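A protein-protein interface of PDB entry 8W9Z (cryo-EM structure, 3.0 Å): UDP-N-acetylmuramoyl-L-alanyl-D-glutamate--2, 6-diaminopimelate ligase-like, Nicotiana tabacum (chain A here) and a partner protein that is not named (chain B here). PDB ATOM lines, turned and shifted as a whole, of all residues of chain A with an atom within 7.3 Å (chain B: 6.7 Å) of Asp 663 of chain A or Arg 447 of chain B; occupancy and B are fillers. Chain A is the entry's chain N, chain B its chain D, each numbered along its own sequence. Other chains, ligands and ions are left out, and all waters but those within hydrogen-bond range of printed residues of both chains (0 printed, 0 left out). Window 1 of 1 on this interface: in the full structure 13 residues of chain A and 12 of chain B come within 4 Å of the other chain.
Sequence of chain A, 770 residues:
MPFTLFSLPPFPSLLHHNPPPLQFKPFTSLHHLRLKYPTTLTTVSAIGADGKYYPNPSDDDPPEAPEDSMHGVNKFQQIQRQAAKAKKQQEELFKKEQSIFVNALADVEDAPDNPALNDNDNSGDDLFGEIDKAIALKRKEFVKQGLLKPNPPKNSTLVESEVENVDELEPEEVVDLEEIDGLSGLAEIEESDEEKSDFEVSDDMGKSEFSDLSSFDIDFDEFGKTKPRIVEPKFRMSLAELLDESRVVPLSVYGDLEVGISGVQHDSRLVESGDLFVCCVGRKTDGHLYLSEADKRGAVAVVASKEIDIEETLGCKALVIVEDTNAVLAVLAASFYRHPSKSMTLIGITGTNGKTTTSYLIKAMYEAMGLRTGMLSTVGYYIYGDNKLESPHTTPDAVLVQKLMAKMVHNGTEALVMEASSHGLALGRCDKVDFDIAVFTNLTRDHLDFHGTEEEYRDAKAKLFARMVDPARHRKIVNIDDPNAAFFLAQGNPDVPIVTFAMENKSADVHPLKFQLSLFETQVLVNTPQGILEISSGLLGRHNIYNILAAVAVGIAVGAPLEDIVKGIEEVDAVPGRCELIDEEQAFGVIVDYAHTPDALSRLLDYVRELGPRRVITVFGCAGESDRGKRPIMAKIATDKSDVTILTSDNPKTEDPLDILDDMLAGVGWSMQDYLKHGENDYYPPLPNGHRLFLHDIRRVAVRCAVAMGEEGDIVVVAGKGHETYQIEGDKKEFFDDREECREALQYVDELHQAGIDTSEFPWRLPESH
O of Arg 628 of chain A sits at hydrogen-bond distance from OH of Tyr 435 of chain B, at 3.1 Å. NH1 of Arg 447 of chain B lies within hydrogen-bond range of O of Asp 659 of chain A (2.7 Å). OD2 of Asp 663 of chain A is in hydrogen-bond range of OH of Tyr 435 of chain B (3.1 Å). The backbone carbonyl oxygen (O) of Trp 448 of chain B sits close to the side-chain amide oxygen (OE1) of Gln 673 of chain A (3.5 Å).
The side-chain carboxylate of Asp 662 of chain A lies within hydrogen-bond range of the backbone NH of Met 672 of chain A (3.1 Å).
Among the printed residues, pairs that only touch across the chains: Gln 673 of chain A with Leu 457 of chain B (3.2 Å), Asp 662 of chain A with Trp 448 of chain B (3.5 Å), Gln 673 of chain A with Val 449 of chain B (3.7 Å), Asp 663 of chain A with Arg 447 of chain B (3.8 Å), Pro 632 of chain A with Tyr 435 of chain B (3.8 Å), Gln 673 of chain A with Pro 450 of chain B (3.9 Å), Ile 660 of chain A with Arg 447 of chain B (3.9 Å) and Ala 666 of chain A with Arg 445 of chain B (3.9995 Å).
Gly 629 of chain A touches none of the printed residues of chain B. Printed residues of chain B within 4 Å of Pro 632 of chain A: Tyr 435 (3.8 Å). Of chain B, only Tyr 435 and Arg 447 come within 4 Å of Asp 663 of chain A. Met 672 of chain A touches none of the printed residues of chain B. Printed residues of chain B within 4 Å of Gln 673 of chain A: Trp 448 (3.2 Å), Val 449 (3.7 Å), Pro 450 (3.9 Å) and Leu 457 (3.2 Å). Of the printed residues of chain A, Tyr 435 of chain B touches Arg 628 (3.1 Å), Pro 632 (3.8 Å) and Asp 663 (3.1 Å). Arg 447 of chain B touches three residues of chain A. Of the printed residues of chain A, Leu 457 of chain B touches Gln 673 (3.2 Å). The nearest residue of chain B that does not touch Asp 663 of chain A is Arg 445 of chain B (5.1 Å).
Hydrophobic or aromatic side chains of chain A within 4 Å of the printed part of chain B: Pro 632 and Ala 666. Of the 11 printed residues of chain B, 7 touch a printed residue of chain A. Printed residues of chain B that touch a printed residue of chain A: Tyr 435, Arg 445, Arg 447, Trp 448, Val 449, Pro 450 and Leu 457. Among the printed residues, no Asp or Glu carboxylate lies within 4 Å of a Lys or Arg side-chain nitrogen of the other chain.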
ATOM      1  N   CYS A 622      -6.119 -10.135 -28.877  1.00  0.00           N
ATOM      2  CA  CYS A 622      -4.796  -9.535 -28.848  1.00  0.00           C
ATOM      3  C   CYS A 622      -3.739 -10.591 -28.557  1.00  0.00           C
ATOM      4  O   CYS A 622      -4.017 -11.638 -27.967  1.00  0.00           O
ATOM      5  CB  CYS A 622      -4.723  -8.418 -27.800  1.00  0.00           C
ATOM      6  SG  CYS A 622      -3.122  -7.583 -27.712  1.00  0.00           S
ATOM      7  N   ASP A 627       2.001  -4.700 -27.801  1.00  0.00           N
ATOM      8  CA  ASP A 627       1.741  -3.324 -27.397  1.00  0.00           C
ATOM      9  C   ASP A 627       0.537  -3.269 -26.467  1.00  0.00           C
ATOM     10  O   ASP A 627      -0.591  -3.553 -26.882  1.00  0.00           O
ATOM     11  CB  ASP A 627       1.516  -2.439 -28.625  1.00  0.00           C
ATOM     12  CG  ASP A 627       1.708  -0.963 -28.328  1.00  0.00           C
ATOM     13  OD1 ASP A 627       1.486  -0.545 -27.173  1.00  0.00           O
ATOM     14  OD2 ASP A 627       2.085  -0.217 -29.257  1.00  0.00           O
ATOM     15  N   ARG A 628       0.768  -2.903 -25.204  1.00  0.00           N
ATOM     16  CA  ARG A 628      -0.319  -2.873 -24.232  1.00  0.00           C
ATOM     17  C   ARG A 628      -1.317  -1.764 -24.536  1.00  0.00           C
ATOM     18  O   ARG A 628      -2.517  -1.927 -24.287  1.00  0.00           O
ATOM     19  CB  ARG A 628       0.243  -2.714 -22.820  1.00  0.00           C
ATOM     20  CG  ARG A 628       1.163  -3.848 -22.392  1.00  0.00           C
ATOM     21  CD  ARG A 628       1.654  -3.655 -20.968  1.00  0.00           C
ATOM     22  NE  ARG A 628       2.521  -4.748 -20.536  1.00  0.00           N
ATOM     23  CZ  ARG A 628       3.080  -4.826 -19.334  1.00  0.00           C
ATOM     24  NH1 ARG A 628       3.856  -5.857 -19.027  1.00  0.00           N
ATOM     25  NH2 ARG A 628       2.866  -3.873 -18.438  1.00  0.00           N
ATOM     26  N   GLY A 629      -0.849  -0.638 -25.073  1.00  0.00           N
ATOM     27  CA  GLY A 629      -1.745   0.439 -25.453  1.00  0.00           C
ATOM     28  C   GLY A 629      -2.561   0.166 -26.697  1.00  0.00           C
ATOM     29  O   GLY A 629      -3.487   0.932 -26.990  1.00  0.00           O
ATOM     30  N   LYS A 630      -2.244  -0.901 -27.432  1.00  0.00           N
ATOM     31  CA  LYS A 630      -2.987  -1.226 -28.643  1.00  0.00           C
ATOM     32  C   LYS A 630      -4.331  -1.874 -28.336  1.00  0.00           C
ATOM     33  O   LYS A 630      -5.291  -1.684 -29.090  1.00  0.00           O
ATOM     34  CB  LYS A 630      -2.152  -2.148 -29.535  1.00  0.00           C
ATOM     35  CG  LYS A 630      -2.759  -2.413 -30.902  1.00  0.00           C
ATOM     36  CD  LYS A 630      -1.928  -3.410 -31.692  1.00  0.00           C
ATOM     37  CE  LYS A 630      -1.849  -4.749 -30.979  1.00  0.00           C
ATOM     38  NZ  LYS A 630      -1.049  -5.742 -31.748  1.00  0.00           N
ATOM     39  N   ARG A 631      -4.420  -2.632 -27.244  1.00  0.00           N
ATOM     40  CA  ARG A 631      -5.670  -3.313 -26.910  1.00  0.00           C
ATOM     41  C   ARG A 631      -6.821  -2.354 -26.621  1.00  0.00           C
ATOM     42  O   ARG A 631      -7.913  -2.556 -27.182  1.00  0.00           O
ATOM     43  CB  ARG A 631      -5.433  -4.267 -25.735  1.00  0.00           C
ATOM     44  N   PRO A 632      -6.673  -1.321 -25.779  1.00  0.00           N
ATOM     45  CA  PRO A 632      -7.844  -0.473 -25.494  1.00  0.00           C
ATOM     46  C   PRO A 632      -8.320   0.318 -26.697  1.00  0.00           C
ATOM     47  O   PRO A 632      -9.533   0.436 -26.907  1.00  0.00           O
ATOM     48  CB  PRO A 632      -7.345   0.442 -24.367  1.00  0.00           C
ATOM     49  CG  PRO A 632      -5.877   0.493 -24.552  1.00  0.00           C
ATOM     50  CD  PRO A 632      -5.492  -0.880 -25.016  1.00  0.00           C
ATOM     51  N   ILE A 633      -7.404   0.864 -27.499  1.00  0.00           N
ATOM     52  CA  ILE A 633      -7.820   1.623 -28.674  1.00  0.00           C
ATOM     53  C   ILE A 633      -8.477   0.704 -29.697  1.00  0.00           C
ATOM     54  O   ILE A 633      -9.454   1.084 -30.354  1.00  0.00           O
ATOM     55  CB  ILE A 633      -6.627   2.396 -29.270  1.00  0.00           C
ATOM     56  CG1 ILE A 633      -7.050   3.155 -30.530  1.00  0.00           C
ATOM     57  CG2 ILE A 633      -5.461   1.463 -29.563  1.00  0.00           C
ATOM     58  CD1 ILE A 633      -8.119   4.197 -30.285  1.00  0.00           C
ATOM     59  N   ALA A 635     -10.182  -2.075 -28.958  1.00  0.00           N
ATOM     60  CA  ALA A 635     -11.507  -2.386 -28.431  1.00  0.00           C
ATOM     61  C   ALA A 635     -12.461  -1.212 -28.611  1.00  0.00           C
ATOM     62  O   ALA A 635     -13.640  -1.404 -28.932  1.00  0.00           O
ATOM     63  CB  ALA A 635     -11.408  -2.777 -26.956  1.00  0.00           C
ATOM     64  N   LEU A 647     -14.893 -10.779 -27.844  1.00  0.00           N
ATOM     65  CA  LEU A 647     -13.486 -10.605 -27.510  1.00  0.00           C
ATOM     66  C   LEU A 647     -12.925 -11.931 -27.016  1.00  0.00           C
ATOM     67  O   LEU A 647     -13.459 -12.523 -26.073  1.00  0.00           O
ATOM     68  CB  LEU A 647     -13.305  -9.512 -26.457  1.00  0.00           C
ATOM     69  CG  LEU A 647     -13.741  -8.107 -26.878  1.00  0.00           C
ATOM     70  CD1 LEU A 647     -13.512  -7.109 -25.754  1.00  0.00           C
ATOM     71  CD2 LEU A 647     -13.008  -7.676 -28.138  1.00  0.00           C
ATOM     72  N   ASP A 656      -0.786 -14.899 -19.543  1.00  0.00           N
ATOM     73  CA  ASP A 656      -1.917 -15.451 -18.808  1.00  0.00           C
ATOM     74  C   ASP A 656      -3.229 -15.045 -19.472  1.00  0.00           C
ATOM     75  O   ASP A 656      -3.414 -13.867 -19.799  1.00  0.00           O
ATOM     76  CB  ASP A 656      -1.888 -14.979 -17.356  1.00  0.00           C
ATOM     77  CG  ASP A 656      -1.651 -13.486 -17.231  1.00  0.00           C
ATOM     78  OD1 ASP A 656      -1.322 -12.846 -18.251  1.00  0.00           O
ATOM     79  OD2 ASP A 656      -1.794 -12.952 -16.111  1.00  0.00           O
ATOM     80  N   LEU A 658      -7.388 -14.280 -19.707  1.00  0.00           N
ATOM     81  CA  LEU A 658      -8.311 -13.491 -18.894  1.00  0.00           C
ATOM     82  C   LEU A 658      -7.635 -12.247 -18.326  1.00  0.00           C
ATOM     83  O   LEU A 658      -8.228 -11.528 -17.516  1.00  0.00           O
ATOM     84  CB  LEU A 658      -8.909 -14.334 -17.761  1.00  0.00           C
ATOM     85  CG  LEU A 658      -9.908 -15.441 -18.115  1.00  0.00           C
ATOM     86  CD1 LEU A 658      -9.209 -16.703 -18.599  1.00  0.00           C
ATOM     87  CD2 LEU A 658     -10.805 -15.748 -16.924  1.00  0.00           C
ATOM     88  N   ASP A 659      -6.395 -11.987 -18.738  1.00  0.00           N
ATOM     89  CA  ASP A 659      -5.665 -10.790 -18.344  1.00  0.00           C
ATOM     90  C   ASP A 659      -5.678  -9.729 -19.438  1.00  0.00           C
ATOM     91  O   ASP A 659      -6.094  -8.593 -19.196  1.00  0.00           O
ATOM     92  CB  ASP A 659      -4.220 -11.147 -17.977  1.00  0.00           C
ATOM     93  N   ILE A 660      -5.226 -10.084 -20.643  1.00  0.00           N
ATOM     94  CA  ILE A 660      -5.350  -9.173 -21.773  1.00  0.00           C
ATOM     95  C   ILE A 660      -6.815  -8.996 -22.148  1.00  0.00           C
ATOM     96  O   ILE A 660      -7.213  -7.937 -22.652  1.00  0.00           O
ATOM     97  CB  ILE A 660      -4.504  -9.681 -22.957  1.00  0.00           C
ATOM     98  CG1 ILE A 660      -4.543  -8.687 -24.120  1.00  0.00           C
ATOM     99  CG2 ILE A 660      -4.966 -11.063 -23.400  1.00  0.00           C
ATOM    100  CD1 ILE A 660      -3.998  -7.318 -23.772  1.00  0.00           C
ATOM    101  N   LEU A 661      -7.642 -10.016 -21.904  1.00  0.00           N
ATOM    102  CA  LEU A 661      -9.078  -9.871 -22.112  1.00  0.00           C
ATOM    103  C   LEU A 661      -9.653  -8.791 -21.205  1.00  0.00           C
ATOM    104  O   LEU A 661     -10.485  -7.983 -21.635  1.00  0.00           O
ATOM    105  CB  LEU A 661      -9.780 -11.208 -21.872  1.00  0.00           C
ATOM    106  CG  LEU A 661     -10.669 -11.719 -23.007  1.00  0.00           C
ATOM    107  CD1 LEU A 661     -11.311 -13.045 -22.631  1.00  0.00           C
ATOM    108  CD2 LEU A 661     -11.726 -10.689 -23.363  1.00  0.00           C
ATOM    109  N   ASP A 662      -9.215  -8.755 -19.944  1.00  0.00           N
ATOM    110  CA  ASP A 662      -9.622  -7.671 -19.058  1.00  0.00           C
ATOM    111  C   ASP A 662      -9.091  -6.329 -19.545  1.00  0.00           C
ATOM    112  O   ASP A 662      -9.754  -5.300 -19.369  1.00  0.00           O
ATOM    113  CB  ASP A 662      -9.146  -7.947 -17.631  1.00  0.00           C
ATOM    114  CG  ASP A 662      -9.653  -6.920 -16.639  1.00  0.00           C
ATOM    115  OD1 ASP A 662     -10.872  -6.910 -16.362  1.00  0.00           O
ATOM    116  OD2 ASP A 662      -8.834  -6.123 -16.136  1.00  0.00           O
ATOM    117  N   ASP A 663      -7.910  -6.320 -20.166  1.00  0.00           N
ATOM    118  CA  ASP A 663      -7.384  -5.085 -20.738  1.00  0.00           C
ATOM    119  C   ASP A 663      -8.286  -4.572 -21.854  1.00  0.00           C
ATOM    120  O   ASP A 663      -8.564  -3.370 -21.935  1.00  0.00           O
ATOM    121  CB  ASP A 663      -5.961  -5.312 -21.250  1.00  0.00           C
ATOM    122  CG  ASP A 663      -5.272  -4.024 -21.659  1.00  0.00           C
ATOM    123  OD1 ASP A 663      -5.827  -2.936 -21.400  1.00  0.00           O
ATOM    124  OD2 ASP A 663      -4.170  -4.101 -22.242  1.00  0.00           O
ATOM    125  N   MET A 664      -8.756  -5.470 -22.722  1.00  0.00           N
ATOM    126  CA  MET A 664      -9.683  -5.060 -23.772  1.00  0.00           C
ATOM    127  C   MET A 664     -11.021  -4.623 -23.188  1.00  0.00           C
ATOM    128  O   MET A 664     -11.646  -3.681 -23.689  1.00  0.00           O
ATOM    129  CB  MET A 664      -9.888  -6.193 -24.779  1.00  0.00           C
ATOM    130  CG  MET A 664      -8.920  -6.174 -25.954  1.00  0.00           C
ATOM    131  SD  MET A 664      -7.470  -7.216 -25.709  1.00  0.00           S
ATOM    132  CE  MET A 664      -8.224  -8.840 -25.656  1.00  0.00           C
ATOM    133  N   LEU A 665     -11.479  -5.298 -22.129  1.00  0.00           N
ATOM    134  CA  LEU A 665     -12.743  -4.921 -21.505  1.00  0.00           C
ATOM    135  C   LEU A 665     -12.658  -3.554 -20.837  1.00  0.00           C
ATOM    136  O   LEU A 665     -13.658  -2.830 -20.783  1.00  0.00           O
ATOM    137  CB  LEU A 665     -13.166  -5.980 -20.489  1.00  0.00           C
ATOM    138  CG  LEU A 665     -14.222  -6.985 -20.952  1.00  0.00           C
ATOM    139  CD1 LEU A 665     -15.524  -6.274 -21.286  1.00  0.00           C
ATOM    140  CD2 LEU A 665     -13.724  -7.783 -22.145  1.00  0.00           C
ATOM    141  N   ALA A 666     -11.482  -3.188 -20.325  1.00  0.00           N
ATOM    142  CA  ALA A 666     -11.318  -1.886 -19.690  1.00  0.00           C
ATOM    143  C   ALA A 666     -11.465  -0.734 -20.674  1.00  0.00           C
ATOM    144  O   ALA A 666     -11.630   0.414 -20.245  1.00  0.00           O
ATOM    145  CB  ALA A 666      -9.956  -1.805 -18.997  1.00  0.00           C
ATOM    146  N   GLY A 667     -11.409  -1.008 -21.979  1.00  0.00           N
ATOM    147  CA  GLY A 667     -11.559   0.057 -22.956  1.00  0.00           C
ATOM    148  C   GLY A 667     -12.954   0.653 -22.964  1.00  0.00           C
ATOM    149  O   GLY A 667     -13.121   1.860 -23.161  1.00  0.00           O
ATOM    150  N   VAL A 668     -13.972  -0.179 -22.754  1.00  0.00           N
ATOM    151  CA  VAL A 668     -15.353   0.289 -22.724  1.00  0.00           C
ATOM    152  C   VAL A 668     -15.730   0.640 -21.292  1.00  0.00           C
ATOM    153  O   VAL A 668     -16.894   0.939 -20.999  1.00  0.00           O
ATOM    154  CB  VAL A 668     -16.315  -0.761 -23.310  1.00  0.00           C
ATOM    155  CG1 VAL A 668     -15.923  -1.102 -24.740  1.00  0.00           C
ATOM    156  CG2 VAL A 668     -16.335  -2.008 -22.441  1.00  0.00           C
ATOM    157  N   TRP A 670     -15.708  -1.384 -18.724  1.00  0.00           N
ATOM    158  CA  TRP A 670     -16.154  -2.541 -17.968  1.00  0.00           C
ATOM    159  C   TRP A 670     -14.963  -3.310 -17.406  1.00  0.00           C
ATOM    160  O   TRP A 670     -13.838  -3.219 -17.900  1.00  0.00           O
ATOM    161  CB  TRP A 670     -17.001  -3.468 -18.841  1.00  0.00           C
ATOM    162  CG  TRP A 670     -18.348  -2.920 -19.191  1.00  0.00           C
ATOM    163  CD1 TRP A 670     -18.819  -1.668 -18.928  1.00  0.00           C
ATOM    164  CD2 TRP A 670     -19.404  -3.613 -19.866  1.00  0.00           C
ATOM    165  NE1 TRP A 670     -20.103  -1.536 -19.400  1.00  0.00           N
ATOM    166  CE2 TRP A 670     -20.485  -2.717 -19.980  1.00  0.00           C
ATOM    167  CE3 TRP A 670     -19.541  -4.904 -20.386  1.00  0.00           C
ATOM    168  CZ2 TRP A 670     -21.686  -3.070 -20.593  1.00  0.00           C
ATOM    169  CZ3 TRP A 670     -20.732  -5.252 -20.994  1.00  0.00           C
ATOM    170  CH2 TRP A 670     -21.789  -4.339 -21.092  1.00  0.00           C
ATOM    171  N   MET A 672     -13.880  -7.370 -15.877  1.00  0.00           N
ATOM    172  CA  MET A 672     -14.298  -8.764 -15.971  1.00  0.00           C
ATOM    173  C   MET A 672     -15.133  -9.184 -14.770  1.00  0.00           C
ATOM    174  O   MET A 672     -16.010 -10.044 -14.897  1.00  0.00           O
ATOM    175  CB  MET A 672     -13.081  -9.676 -16.117  1.00  0.00           C
ATOM    176  CG  MET A 672     -12.425  -9.613 -17.483  1.00  0.00           C
ATOM    177  SD  MET A 672     -11.317 -11.002 -17.780  1.00  0.00           S
ATOM    178  CE  MET A 672     -12.455 -12.377 -17.632  1.00  0.00           C
ATOM    179  N   GLN A 673     -14.882  -8.586 -13.604  1.00  0.00           N
ATOM    180  CA  GLN A 673     -15.681  -8.904 -12.425  1.00  0.00           C
ATOM    181  C   GLN A 673     -17.138  -8.509 -12.624  1.00  0.00           C
ATOM    182  O   GLN A 673     -18.049  -9.257 -12.252  1.00  0.00           O
ATOM    183  CB  GLN A 673     -15.097  -8.208 -11.197  1.00  0.00           C
ATOM    184  CG  GLN A 673     -13.617  -8.466 -10.994  1.00  0.00           C
ATOM    185  CD  GLN A 673     -13.030  -7.640  -9.872  1.00  0.00           C
ATOM    186  OE1 GLN A 673     -11.817  -7.620  -9.671  1.00  0.00           O
ATOM    187  NE2 GLN A 673     -13.890  -6.949  -9.133  1.00  0.00           N
ATOM    188  N   TYR B 435      -6.409   4.568 -18.695  1.00  0.00           N
ATOM    189  CA  TYR B 435      -5.606   3.351 -18.743  1.00  0.00           C
ATOM    190  C   TYR B 435      -4.119   3.672 -18.812  1.00  0.00           C
ATOM    191  O   TYR B 435      -3.304   3.010 -18.160  1.00  0.00           O
ATOM    192  CB  TYR B 435      -6.028   2.494 -19.937  1.00  0.00           C
ATOM    193  CG  TYR B 435      -5.070   1.370 -20.259  1.00  0.00           C
ATOM    194  CD1 TYR B 435      -5.071   0.197 -19.517  1.00  0.00           C
ATOM    195  CD2 TYR B 435      -4.169   1.480 -21.310  1.00  0.00           C
ATOM    196  CE1 TYR B 435      -4.197  -0.832 -19.808  1.00  0.00           C
ATOM    197  CE2 TYR B 435      -3.291   0.456 -21.608  1.00  0.00           C
ATOM    198  CZ  TYR B 435      -3.310  -0.698 -20.855  1.00  0.00           C
ATOM    199  OH  TYR B 435      -2.438  -1.722 -21.148  1.00  0.00           O
ATOM    200  N   GLY B 440      -0.319   0.391 -17.438  1.00  0.00           N
ATOM    201  CA  GLY B 440      -0.224  -0.062 -18.813  1.00  0.00           C
ATOM    202  C   GLY B 440       1.024   0.394 -19.541  1.00  0.00           C
ATOM    203  O   GLY B 440       1.661   1.376 -19.148  1.00  0.00           O
ATOM    204  N   ASP B 444       3.492  -3.283 -14.430  1.00  0.00           N
ATOM    205  CA  ASP B 444       2.316  -4.112 -14.220  1.00  0.00           C
ATOM    206  C   ASP B 444       1.144  -3.224 -13.826  1.00  0.00           C
ATOM    207  O   ASP B 444       1.318  -2.190 -13.177  1.00  0.00           O
ATOM    208  CB  ASP B 444       2.562  -5.177 -13.140  1.00  0.00           C
ATOM    209  CG  ASP B 444       1.564  -6.320 -13.204  1.00  0.00           C
ATOM    210  OD1 ASP B 444       0.442  -6.114 -13.712  1.00  0.00           O
ATOM    211  OD2 ASP B 444       1.904  -7.430 -12.742  1.00  0.00           O
ATOM    212  N   ARG B 445      -0.053  -3.641 -14.229  1.00  0.00           N
ATOM    213  CA  ARG B 445      -1.284  -2.922 -13.939  1.00  0.00           C
ATOM    214  C   ARG B 445      -2.180  -3.785 -13.063  1.00  0.00           C
ATOM    215  O   ARG B 445      -2.211  -5.011 -13.210  1.00  0.00           O
ATOM    216  CB  ARG B 445      -2.014  -2.539 -15.232  1.00  0.00           C
ATOM    217  CG  ARG B 445      -3.331  -1.808 -15.023  1.00  0.00           C
ATOM    218  CD  ARG B 445      -4.001  -1.486 -16.347  1.00  0.00           C
ATOM    219  NE  ARG B 445      -5.295  -0.836 -16.162  1.00  0.00           N
ATOM    220  CZ  ARG B 445      -6.453  -1.484 -16.103  1.00  0.00           C
ATOM    221  NH1 ARG B 445      -7.584  -0.811 -15.934  1.00  0.00           N
ATOM    222  NH2 ARG B 445      -6.484  -2.804 -16.216  1.00  0.00           N
ATOM    223  N   LYS B 446      -2.907  -3.142 -12.154  1.00  0.00           N
ATOM    224  CA  LYS B 446      -3.818  -3.849 -11.255  1.00  0.00           C
ATOM    225  C   LYS B 446      -4.999  -4.360 -12.068  1.00  0.00           C
ATOM    226  O   LYS B 446      -5.925  -3.611 -12.386  1.00  0.00           O
ATOM    227  CB  LYS B 446      -4.274  -2.929 -10.128  1.00  0.00           C
ATOM    228  N   ARG B 447      -4.968  -5.644 -12.412  1.00  0.00           N
ATOM    229  CA  ARG B 447      -5.998  -6.255 -13.242  1.00  0.00           C
ATOM    230  C   ARG B 447      -7.116  -6.788 -12.354  1.00  0.00           C
ATOM    231  O   ARG B 447      -6.888  -7.672 -11.521  1.00  0.00           O
ATOM    232  CB  ARG B 447      -5.406  -7.373 -14.097  1.00  0.00           C
ATOM    233  CG  ARG B 447      -4.291  -6.914 -15.021  1.00  0.00           C
ATOM    234  CD  ARG B 447      -3.764  -8.058 -15.869  1.00  0.00           C
ATOM    235  NE  ARG B 447      -2.679  -7.628 -16.746  1.00  0.00           N
ATOM    236  CZ  ARG B 447      -2.857  -7.132 -17.965  1.00  0.00           C
ATOM    237  NH1 ARG B 447      -4.081  -7.000 -18.457  1.00  0.00           N
ATOM    238  NH2 ARG B 447      -1.811  -6.766 -18.694  1.00  0.00           N
ATOM    239  N   TRP B 448      -8.322  -6.254 -12.540  1.00  0.00           N
ATOM    240  CA  TRP B 448      -9.492  -6.662 -11.763  1.00  0.00           C
ATOM    241  C   TRP B 448     -10.028  -7.971 -12.337  1.00  0.00           C
ATOM    242  O   TRP B 448     -11.039  -8.018 -13.040  1.00  0.00           O
ATOM    243  CB  TRP B 448     -10.552  -5.568 -11.779  1.00  0.00           C
ATOM    244  CG  TRP B 448     -10.110  -4.285 -11.146  1.00  0.00           C
ATOM    245  CD1 TRP B 448      -9.277  -3.349 -11.686  1.00  0.00           C
ATOM    246  CD2 TRP B 448     -10.486  -3.790  -9.856  1.00  0.00           C
ATOM    247  NE1 TRP B 448      -9.106  -2.305 -10.810  1.00  0.00           N
ATOM    248  CE2 TRP B 448      -9.839  -2.551  -9.679  1.00  0.00           C
ATOM    249  CE3 TRP B 448     -11.306  -4.276  -8.833  1.00  0.00           C
ATOM    250  CZ2 TRP B 448      -9.986  -1.792  -8.521  1.00  0.00           C
ATOM    251  CZ3 TRP B 448     -11.449  -3.520  -7.683  1.00  0.00           C
ATOM    252  CH2 TRP B 448     -10.794  -2.292  -7.537  1.00  0.00           C
ATOM    253  N   VAL B 449      -9.331  -9.057 -12.020  1.00  0.00           N
ATOM    254  CA  VAL B 449      -9.673 -10.391 -12.495  1.00  0.00           C
ATOM    255  C   VAL B 449      -9.830 -11.298 -11.282  1.00  0.00           C
ATOM    256  O   VAL B 449      -8.939 -11.336 -10.432  1.00  0.00           O
ATOM    257  CB  VAL B 449      -8.617 -10.962 -13.461  1.00  0.00           C
ATOM    258  CG1 VAL B 449      -7.211 -10.681 -12.948  1.00  0.00           C
ATOM    259  CG2 VAL B 449      -8.829 -12.454 -13.662  1.00  0.00           C
ATOM    260  N   PRO B 450     -10.939 -12.022 -11.150  1.00  0.00           N
ATOM    261  CA  PRO B 450     -11.095 -12.926 -10.004  1.00  0.00           C
ATOM    262  C   PRO B 450     -10.147 -14.110 -10.094  1.00  0.00           C
ATOM    263  O   PRO B 450      -9.845 -14.609 -11.181  1.00  0.00           O
ATOM    264  CB  PRO B 450     -12.559 -13.374 -10.100  1.00  0.00           C
ATOM    265  CG  PRO B 450     -13.223 -12.356 -10.975  1.00  0.00           C
ATOM    266  CD  PRO B 450     -12.172 -11.923 -11.946  1.00  0.00           C
ATOM    267  N   ARG B 451      -9.677 -14.558  -8.933  1.00  0.00           N
ATOM    268  CA  ARG B 451      -8.783 -15.701  -8.829  1.00  0.00           C
ATOM    269  C   ARG B 451      -9.326 -16.674  -7.791  1.00  0.00           C
ATOM    270  O   ARG B 451     -10.335 -16.416  -7.129  1.00  0.00           O
ATOM    271  CB  ARG B 451      -7.356 -15.268  -8.467  1.00  0.00           C
ATOM    272  CG  ARG B 451      -6.672 -14.444  -9.543  1.00  0.00           C
ATOM    273  CD  ARG B 451      -6.584 -15.215 -10.849  1.00  0.00           C
ATOM    274  NE  ARG B 451      -5.953 -14.431 -11.908  1.00  0.00           N
ATOM    275  CZ  ARG B 451      -5.773 -14.865 -13.151  1.00  0.00           C
ATOM    276  NH1 ARG B 451      -6.175 -16.080 -13.497  1.00  0.00           N
ATOM    277  NH2 ARG B 451      -5.189 -14.083 -14.050  1.00  0.00           N
ATOM    278  N   LEU B 457      -9.220  -9.111  -2.970  1.00  0.00           N
ATOM    279  CA  LEU B 457      -9.217  -8.631  -4.349  1.00  0.00           C
ATOM    280  C   LEU B 457      -9.185  -7.108  -4.403  1.00  0.00           C
ATOM    281  O   LEU B 457      -8.344  -6.520  -5.091  1.00  0.00           O
ATOM    282  CB  LEU B 457     -10.439  -9.180  -5.087  1.00  0.00           C
ATOM    283  CG  LEU B 457     -10.721  -8.672  -6.501  1.00  0.00           C
ATOM    284  CD1 LEU B 457     -11.138  -9.827  -7.394  1.00  0.00           C
ATOM    285  CD2 LEU B 457     -11.804  -7.604  -6.472  1.00  0.00           C
